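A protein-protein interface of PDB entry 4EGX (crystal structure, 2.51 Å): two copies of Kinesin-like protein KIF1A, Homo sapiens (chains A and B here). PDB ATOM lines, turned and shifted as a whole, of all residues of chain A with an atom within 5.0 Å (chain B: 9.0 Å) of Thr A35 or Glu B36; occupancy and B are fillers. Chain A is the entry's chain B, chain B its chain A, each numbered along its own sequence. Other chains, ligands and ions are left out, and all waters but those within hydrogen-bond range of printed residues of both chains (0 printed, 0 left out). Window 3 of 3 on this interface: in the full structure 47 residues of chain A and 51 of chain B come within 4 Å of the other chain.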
ATOM      1  N   LYS A  31     -34.316  29.818 -13.596  1.00  0.00           N
ATOM      2  CA  LYS A  31     -33.276  29.037 -12.928  1.00  0.00           C
ATOM      3  C   LYS A  31     -32.395  28.343 -13.953  1.00  0.00           C
ATOM      4  O   LYS A  31     -31.195  28.581 -13.998  1.00  0.00           O
ATOM      5  CB  LYS A  31     -33.879  27.994 -11.979  1.00  0.00           C
ATOM      6  CG  LYS A  31     -34.467  28.527 -10.686  1.00  0.00           C
ATOM      7  CD  LYS A  31     -34.723  27.372  -9.721  1.00  0.00           C
ATOM      8  CE  LYS A  31     -35.474  27.808  -8.448  1.00  0.00           C
ATOM      9  NZ  LYS A  31     -35.399  26.756  -7.373  1.00  0.00           N
ATOM     10  N   LEU A  32     -33.012  27.498 -14.773  1.00  0.00           N
ATOM     11  CA  LEU A  32     -32.323  26.724 -15.802  1.00  0.00           C
ATOM     12  C   LEU A  32     -31.475  27.596 -16.730  1.00  0.00           C
ATOM     13  O   LEU A  32     -30.429  27.154 -17.217  1.00  0.00           O
ATOM     14  CB  LEU A  32     -33.351  25.914 -16.610  1.00  0.00           C
ATOM     15  CG  LEU A  32     -32.994  24.822 -17.638  1.00  0.00           C
ATOM     16  CD1 LEU A  32     -32.721  25.374 -19.056  1.00  0.00           C
ATOM     17  CD2 LEU A  32     -31.858  23.906 -17.173  1.00  0.00           C
ATOM     18  N   ARG A  33     -31.922  28.835 -16.943  1.00  0.00           N
ATOM     19  CA  ARG A  33     -31.293  29.776 -17.873  1.00  0.00           C
ATOM     20  C   ARG A  33     -29.933  30.315 -17.380  1.00  0.00           C
ATOM     21  O   ARG A  33     -28.940  30.269 -18.115  1.00  0.00           O
ATOM     22  CB  ARG A  33     -32.279  30.905 -18.157  1.00  0.00           C
ATOM     23  CG  ARG A  33     -31.727  32.129 -18.832  1.00  0.00           C
ATOM     24  CD  ARG A  33     -32.744  33.243 -18.714  1.00  0.00           C
ATOM     25  NE  ARG A  33     -34.058  32.806 -19.180  1.00  0.00           N
ATOM     26  CZ  ARG A  33     -35.211  33.225 -18.669  1.00  0.00           C
ATOM     27  NH1 ARG A  33     -35.228  34.092 -17.660  1.00  0.00           N
ATOM     28  NH2 ARG A  33     -36.353  32.764 -19.162  1.00  0.00           N
ATOM     29  N   ARG A  34     -29.896  30.828 -16.148  1.00  0.00           N
ATOM     30  CA  ARG A  34     -28.634  31.209 -15.509  1.00  0.00           C
ATOM     31  C   ARG A  34     -27.738  29.983 -15.431  1.00  0.00           C
ATOM     32  O   ARG A  34     -26.611  29.997 -15.893  1.00  0.00           O
ATOM     33  CB  ARG A  34     -28.865  31.715 -14.088  1.00  0.00           C
ATOM     34  CG  ARG A  34     -29.767  32.910 -13.955  1.00  0.00           C
ATOM     35  CD  ARG A  34     -29.676  33.440 -12.522  1.00  0.00           C
ATOM     36  NE  ARG A  34     -30.850  34.165 -12.015  1.00  0.00           N
ATOM     37  CZ  ARG A  34     -31.962  34.484 -12.706  1.00  0.00           C
ATOM     38  NH1 ARG A  34     -32.133  34.158 -14.003  1.00  0.00           N
ATOM     39  NH2 ARG A  34     -32.919  35.154 -12.074  1.00  0.00           N
ATOM     40  N   THR A  35     -28.284  28.927 -14.833  1.00  0.00           N
ATOM     41  CA  THR A  35     -27.631  27.629 -14.661  1.00  0.00           C
ATOM     42  C   THR A  35     -26.877  27.137 -15.893  1.00  0.00           C
ATOM     43  O   THR A  35     -25.750  26.618 -15.775  1.00  0.00           O
ATOM     44  CB  THR A  35     -28.677  26.589 -14.275  1.00  0.00           C
ATOM     45  OG1 THR A  35     -29.479  27.120 -13.212  1.00  0.00           O
ATOM     46  CG2 THR A  35     -28.023  25.307 -13.822  1.00  0.00           C
ATOM     47  N   GLU A  36     -27.497  27.288 -17.063  1.00  0.00           N
ATOM     48  CA  GLU A  36     -26.825  27.022 -18.332  1.00  0.00           C
ATOM     49  C   GLU A  36     -25.746  28.072 -18.631  1.00  0.00           C
ATOM     50  O   GLU A  36     -24.683  27.740 -19.156  1.00  0.00           O
ATOM     51  CB  GLU A  36     -27.841  26.949 -19.480  1.00  0.00           C
ATOM     52  N   ALA A  37     -26.024  29.332 -18.288  1.00  0.00           N
ATOM     53  CA  ALA A  37     -25.097  30.450 -18.552  1.00  0.00           C
ATOM     54  C   ALA A  37     -23.841  30.415 -17.669  1.00  0.00           C
ATOM     55  O   ALA A  37     -22.793  30.958 -18.039  1.00  0.00           O
ATOM     56  CB  ALA A  37     -25.817  31.797 -18.412  1.00  0.00           C
ATOM     57  N   ILE A  38     -23.957  29.784 -16.502  1.00  0.00           N
ATOM     58  CA  ILE A  38     -22.795  29.504 -15.669  1.00  0.00           C
ATOM     59  C   ILE A  38     -21.945  28.443 -16.370  1.00  0.00           C
ATOM     60  O   ILE A  38     -20.721  28.496 -16.333  1.00  0.00           O
ATOM     61  CB  ILE A  38     -23.176  29.023 -14.244  1.00  0.00           C
ATOM     62  CG1 ILE A  38     -24.182  29.964 -13.574  1.00  0.00           C
ATOM     63  CG2 ILE A  38     -21.939  28.933 -13.369  1.00  0.00           C
ATOM     64  CD1 ILE A  38     -24.681  29.461 -12.222  1.00  0.00           C
ATOM     65  N   ARG A  39     -22.613  27.483 -17.007  1.00  0.00           N
ATOM     66  CA  ARG A  39     -21.954  26.449 -17.806  1.00  0.00           C
ATOM     67  C   ARG A  39     -21.461  27.021 -19.153  1.00  0.00           C
ATOM     68  O   ARG A  39     -20.584  26.438 -19.810  1.00  0.00           O
ATOM     69  CB  ARG A  39     -22.896  25.246 -17.989  1.00  0.00           C
ATOM     70  CG  ARG A  39     -22.356  24.094 -18.835  1.00  0.00           C
ATOM     71  CD  ARG A  39     -23.514  23.296 -19.412  1.00  0.00           C
ATOM     72  NE  ARG A  39     -23.386  23.073 -20.854  1.00  0.00           N
ATOM     73  CZ  ARG A  39     -23.601  24.001 -21.787  1.00  0.00           C
ATOM     74  NH1 ARG A  39     -23.936  25.245 -21.448  1.00  0.00           N
ATOM     75  NH2 ARG A  39     -23.468  23.689 -23.068  1.00  0.00           N
ATOM     76  N   TRP B  28     -39.290  19.598 -13.352  1.00  0.00           N
ATOM     77  CA  TRP B  28     -38.420  20.755 -13.432  1.00  0.00           C
ATOM     78  C   TRP B  28     -37.189  20.582 -12.547  1.00  0.00           C
ATOM     79  O   TRP B  28     -36.070  20.878 -12.974  1.00  0.00           O
ATOM     80  CB  TRP B  28     -39.164  22.019 -13.032  1.00  0.00           C
ATOM     81  CG  TRP B  28     -39.669  22.833 -14.168  1.00  0.00           C
ATOM     82  CD1 TRP B  28     -40.956  23.227 -14.376  1.00  0.00           C
ATOM     83  CD2 TRP B  28     -38.897  23.383 -15.246  1.00  0.00           C
ATOM     84  NE1 TRP B  28     -41.038  23.985 -15.517  1.00  0.00           N
ATOM     85  CE2 TRP B  28     -39.791  24.096 -16.073  1.00  0.00           C
ATOM     86  CE3 TRP B  28     -37.538  23.341 -15.592  1.00  0.00           C
ATOM     87  CZ2 TRP B  28     -39.377  24.753 -17.232  1.00  0.00           C
ATOM     88  CZ3 TRP B  28     -37.126  23.997 -16.747  1.00  0.00           C
ATOM     89  CH2 TRP B  28     -38.045  24.693 -17.553  1.00  0.00           C
ATOM     90  N   GLU B  29     -37.404  20.101 -11.322  1.00  0.00           N
ATOM     91  CA  GLU B  29     -36.326  19.871 -10.366  1.00  0.00           C
ATOM     92  C   GLU B  29     -35.394  18.773 -10.848  1.00  0.00           C
ATOM     93  O   GLU B  29     -34.205  18.757 -10.508  1.00  0.00           O
ATOM     94  CB  GLU B  29     -36.900  19.502  -9.000  1.00  0.00           C
ATOM     95  CG  GLU B  29     -35.843  19.063  -7.977  1.00  0.00           C
ATOM     96  CD  GLU B  29     -36.248  19.383  -6.554  1.00  0.00           C
ATOM     97  OE1 GLU B  29     -37.382  19.887  -6.356  1.00  0.00           O
ATOM     98  OE2 GLU B  29     -35.425  19.139  -5.632  1.00  0.00           O
ATOM     99  N   GLU B  30     -35.957  17.865 -11.642  1.00  0.00           N
ATOM    100  CA  GLU B  30     -35.243  16.721 -12.193  1.00  0.00           C
ATOM    101  C   GLU B  30     -34.353  17.185 -13.329  1.00  0.00           C
ATOM    102  O   GLU B  30     -33.196  16.777 -13.429  1.00  0.00           O
ATOM    103  CB  GLU B  30     -36.250  15.677 -12.693  1.00  0.00           C
ATOM    104  CG  GLU B  30     -35.793  14.244 -12.548  1.00  0.00           C
ATOM    105  CD  GLU B  30     -34.822  13.842 -13.626  1.00  0.00           C
ATOM    106  OE1 GLU B  30     -35.047  14.246 -14.785  1.00  0.00           O
ATOM    107  OE2 GLU B  30     -33.840  13.130 -13.314  1.00  0.00           O
ATOM    108  N   LYS B  31     -34.905  18.047 -14.177  1.00  0.00           N
ATOM    109  CA  LYS B  31     -34.146  18.675 -15.247  1.00  0.00           C
ATOM    110  C   LYS B  31     -33.065  19.589 -14.672  1.00  0.00           C
ATOM    111  O   LYS B  31     -31.935  19.596 -15.164  1.00  0.00           O
ATOM    112  CB  LYS B  31     -35.075  19.453 -16.184  1.00  0.00           C
ATOM    113  N   LEU B  32     -33.411  20.338 -13.623  1.00  0.00           N
ATOM    114  CA  LEU B  32     -32.459  21.220 -12.939  1.00  0.00           C
ATOM    115  C   LEU B  32     -31.326  20.413 -12.295  1.00  0.00           C
ATOM    116  O   LEU B  32     -30.157  20.782 -12.430  1.00  0.00           O
ATOM    117  CB  LEU B  32     -33.175  22.096 -11.898  1.00  0.00           C
ATOM    118  CG  LEU B  32     -32.852  23.602 -11.775  1.00  0.00           C
ATOM    119  CD1 LEU B  32     -31.700  23.891 -10.809  1.00  0.00           C
ATOM    120  CD2 LEU B  32     -32.600  24.254 -13.137  1.00  0.00           C
ATOM    121  N   ARG B  33     -31.676  19.310 -11.620  1.00  0.00           N
ATOM    122  CA  ARG B  33     -30.685  18.373 -11.063  1.00  0.00           C
ATOM    123  C   ARG B  33     -29.691  17.883 -12.119  1.00  0.00           C
ATOM    124  O   ARG B  33     -28.476  17.999 -11.920  1.00  0.00           O
ATOM    125  CB  ARG B  33     -31.363  17.159 -10.410  1.00  0.00           C
ATOM    126  CG  ARG B  33     -31.736  17.314  -8.930  1.00  0.00           C
ATOM    127  CD  ARG B  33     -32.274  16.003  -8.358  1.00  0.00           C
ATOM    128  N   ARG B  34     -30.217  17.353 -13.233  1.00  0.00           N
ATOM    129  CA  ARG B  34     -29.409  16.828 -14.354  1.00  0.00           C
ATOM    130  C   ARG B  34     -28.471  17.858 -14.960  1.00  0.00           C
ATOM    131  O   ARG B  34     -27.334  17.536 -15.297  1.00  0.00           O
ATOM    132  CB  ARG B  34     -30.304  16.293 -15.476  1.00  0.00           C
ATOM    133  CG  ARG B  34     -30.459  14.774 -15.558  1.00  0.00           C
ATOM    134  CD  ARG B  34     -31.349  14.396 -16.743  1.00  0.00           C
ATOM    135  NE  ARG B  34     -32.717  14.901 -16.563  1.00  0.00           N
ATOM    136  CZ  ARG B  34     -33.577  15.167 -17.549  1.00  0.00           C
ATOM    137  NH1 ARG B  34     -33.235  14.998 -18.823  1.00  0.00           N
ATOM    138  NH2 ARG B  34     -34.793  15.617 -17.253  1.00  0.00           N
ATOM    139  N   THR B  35     -28.959  19.086 -15.104  1.00  0.00           N
ATOM    140  CA  THR B  35     -28.223  20.155 -15.779  1.00  0.00           C
ATOM    141  C   THR B  35     -27.137  20.792 -14.894  1.00  0.00           C
ATOM    142  O   THR B  35     -26.006  20.986 -15.345  1.00  0.00           O
ATOM    143  CB  THR B  35     -29.196  21.229 -16.320  1.00  0.00           C
ATOM    144  OG1 THR B  35     -30.326  20.581 -16.914  1.00  0.00           O
ATOM    145  CG2 THR B  35     -28.525  22.127 -17.375  1.00  0.00           C
ATOM    146  N   GLU B  36     -27.486  21.098 -13.644  1.00  0.00           N
ATOM    147  CA  GLU B  36     -26.530  21.615 -12.658  1.00  0.00           C
ATOM    148  C   GLU B  36     -25.333  20.680 -12.451  1.00  0.00           C
ATOM    149  O   GLU B  36     -24.239  21.133 -12.113  1.00  0.00           O
ATOM    150  CB  GLU B  36     -27.220  21.849 -11.307  1.00  0.00           C
ATOM    151  CG  GLU B  36     -28.295  22.935 -11.317  1.00  0.00           C
ATOM    152  N   ALA B  37     -25.556  19.379 -12.647  1.00  0.00           N
ATOM    153  CA  ALA B  37     -24.514  18.364 -12.476  1.00  0.00           C
ATOM    154  C   ALA B  37     -23.463  18.376 -13.593  1.00  0.00           C
ATOM    155  O   ALA B  37     -22.319  17.993 -13.357  1.00  0.00           O
ATOM    156  CB  ALA B  37     -25.132  16.975 -12.335  1.00  0.00           C
ATOM    157  N   ILE B  38     -23.857  18.806 -14.795  1.00  0.00           N
ATOM    158  CA  ILE B  38     -22.922  19.024 -15.901  1.00  0.00           C
ATOM    159  C   ILE B  38     -21.955  20.142 -15.517  1.00  0.00           C
ATOM    160  O   ILE B  38     -20.738  20.014 -15.685  1.00  0.00           O
ATOM    161  CB  ILE B  38     -23.652  19.387 -17.222  1.00  0.00           C
ATOM    162  CG1 ILE B  38     -24.679  18.313 -17.573  1.00  0.00           C
ATOM    163  CG2 ILE B  38     -22.660  19.556 -18.373  1.00  0.00           C
ATOM    164  CD1 ILE B  38     -25.478  18.582 -18.851  1.00  0.00           C
ATOM    165  N   ARG B  39     -22.518  21.229 -14.991  1.00  0.00           N
ATOM    166  CA  ARG B  39     -21.758  22.384 -14.514  1.00  0.00           C
ATOM    167  C   ARG B  39     -20.788  21.954 -13.431  1.00  0.00           C
ATOM    168  O   ARG B  39     -19.616  22.316 -13.465  1.00  0.00           O
ATOM    169  CB  ARG B  39     -22.708  23.433 -13.936  1.00  0.00           C
ATOM    170  CG  ARG B  39     -22.197  24.862 -14.017  1.00  0.00           C
ATOM    171  CD  ARG B  39     -22.556  25.696 -12.762  1.00  0.00           C
ATOM    172  NE  ARG B  39     -23.693  25.189 -11.989  1.00  0.00           N
ATOM    173  CZ  ARG B  39     -23.599  24.727 -10.741  1.00  0.00           C
ATOM    174  NH1 ARG B  39     -22.424  24.717 -10.109  1.00  0.00           N
ATOM    175  NH2 ARG B  39     -24.684  24.279 -10.118  1.00  0.00           N
ATOM    176  N   MET B  40     -21.297  21.172 -12.477  1.00  0.00           N
ATOM    177  CA  MET B  40     -20.497  20.669 -11.364  1.00  0.00           C
ATOM    178  C   MET B  40     -19.421  19.675 -11.807  1.00  0.00           C
ATOM    179  O   MET B  40     -18.386  19.559 -11.151  1.00  0.00           O
ATOM    180  CB  MET B  40     -21.395  20.095 -10.260  1.00  0.00           C
ATOM    181  CG  MET B  40     -22.189  21.177  -9.515  1.00  0.00           C
ATOM    182  SD  MET B  40     -23.164  20.579  -8.112  1.00  0.00           S
ATOM    183  CE  MET B  40     -23.872  22.118  -7.474  1.00  0.00           C
ATOM    184  N   GLU B  41     -19.661  18.989 -12.927  1.00  0.00           N
ATOM    185  CA  GLU B  41     -18.670  18.104 -13.546  1.00  0.00           C
ATOM    186  C   GLU B  41     -17.565  18.885 -14.264  1.00  0.00           C
ATOM    187  O   GLU B  41     -16.407  18.477 -14.247  1.00  0.00           O
ATOM    188  CB  GLU B  41     -19.328  17.153 -14.537  1.00  0.00           C
ATOM    189  CG  GLU B  41     -20.162  16.035 -13.925  1.00  0.00           C
ATOM    190  CD  GLU B  41     -21.071  15.385 -14.961  1.00  0.00           C
ATOM    191  OE1 GLU B  41     -20.811  15.603 -16.171  1.00  0.00           O
ATOM    192  OE2 GLU B  41     -22.040  14.678 -14.577  1.00  0.00           O
ATOM    193  N   ARG B  42     -17.931  19.992 -14.912  1.00  0.00           N
ATOM    194  CA  ARG B  42     -16.945  20.916 -15.482  1.00  0.00           C
ATOM    195  C   ARG B  42     -16.166  21.622 -14.367  1.00  0.00           C
ATOM    196  O   ARG B  42     -14.956  21.842 -14.484  1.00  0.00           O
ATOM    197  CB  ARG B  42     -17.628  21.953 -16.364  1.00  0.00           C
ATOM    198  CG  ARG B  42     -18.607  21.374 -17.354  1.00  0.00           C
ATOM    199  CD  ARG B  42     -17.960  20.979 -18.673  1.00  0.00           C
ATOM    200  NE  ARG B  42     -18.956  20.941 -19.747  1.00  0.00           N
ATOM    201  CZ  ARG B  42     -19.342  22.006 -20.442  1.00  0.00           C
ATOM    202  NH1 ARG B  42     -18.810  23.192 -20.186  1.00  0.00           N
ATOM    203  NH2 ARG B  42     -20.255  21.889 -21.397  1.00  0.00           N
ATOM    204  N   GLU B  43     -16.872  21.975 -13.295  1.00  0.00           N
ATOM    205  CA  GLU B  43     -16.262  22.529 -12.085  1.00  0.00           C
ATOM    206  C   GLU B  43     -15.350  21.513 -11.401  1.00  0.00           C
ATOM    207  O   GLU B  43     -14.455  21.895 -10.647  1.00  0.00           O
ATOM    208  CB  GLU B  43     -17.343  22.996 -11.099  1.00  0.00           C
ATOM    209  CG  GLU B  43     -18.010  24.303 -11.488  1.00  0.00           C
ATOM    210  CD  GLU B  43     -19.192  24.686 -10.601  1.00  0.00           C
ATOM    211  OE1 GLU B  43     -19.519  23.944  -9.652  1.00  0.00           O
ATOM    212  OE2 GLU B  43     -19.797  25.749 -10.859  1.00  0.00           O
ATOM    213  N   ALA B  44     -15.607  20.225 -11.653  1.00  0.00           N
ATOM    214  CA  ALA B  44     -14.777  19.145 -11.134  1.00  0.00           C
ATOM    215  C   ALA B  44     -13.571  18.969 -12.045  1.00  0.00           C
ATOM    216  O   ALA B  44     -12.470  18.667 -11.574  1.00  0.00           O
ATOM    217  CB  ALA B  44     -15.572  17.842 -11.035  1.00  0.00           C
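Among the printed residues, merely in contact across the chains: Ile A38 with Arg B39, Thr A35 with Glu B36, Leu A32 with Leu B32, Leu A32 with Thr B35, Arg A39 with Ile B38 and Arg A39 with Arg B39.
Leu A32 touches its own counterpart, Leu B32.
Leu A32 touches Thr B35, but with the chains exchanged Thr A35 does not touch Leu B32 (4.2 Å).
Thr A35 touches Glu B36, but with the chains exchanged Glu A36 does not touch Thr B35 (5.3 Å).
Ile A38 touches Arg B39, and with the chains exchanged Arg A39 touches Ile B38.
Of the 7 pairs that touch across the chains among the printed residues, 4 have their exchanged pair printed and touching as well.
Of the 17 printed residues of chain B, 6 touch a printed residue of chain A.
Printed residues of chain A that touch a printed residue of chain B: Leu A32, Thr A35, Ile A38 and Arg A39.
Among the printed residues, 7 pairs touch across the chains.
Among the printed residues, no Asp or Glu carboxylate lies within 4 Å of a Lys or Arg side-chain nitrogen of the other chain.
The guanidinium group of Arg A39 sits close to the guanidinium group of Arg B42 (3.4 Å).
Printed residues of chain B within 4 Å of Leu A32: Leu B32 (3.6 Å) and Thr B35 (3.7 Å).
Thr A35 touches just one residue of chain B: Glu B36 (3.5 Å).
No residue of chain B comes within 4 Å of Glu A36.
Printed residues of chain A within 4 Å of Leu B32: Leu A32 (3.6 Å).
Of the printed residues of chain A, Thr B35 touches Leu A32 (3.7 Å).
Of chain A, only Thr A35 comes within 4 Å of Glu B36.
Of the printed residues of chain A, Ile B38 touches Arg A39.
Printed residues of chain A within 4 Å of Arg B39: Ile A38 and Arg A39.
Ala B44 touches none of the printed residues of chain A.
The nearest residue of chain B that does not touch Thr A35 is Leu B32 (4.2 Å).
The backbone carbonyl oxygen (O) of Lys B31 sits at hydrogen-bond distance from the side-chain hydroxyl (OG1) of Thr B35 (2.6 Å).
OE2 of Glu B43 is in salt-bridge range of NH1 of Arg B39.
NH1 of Arg A39 lies close to O of Glu A36, at 3.5 Å.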
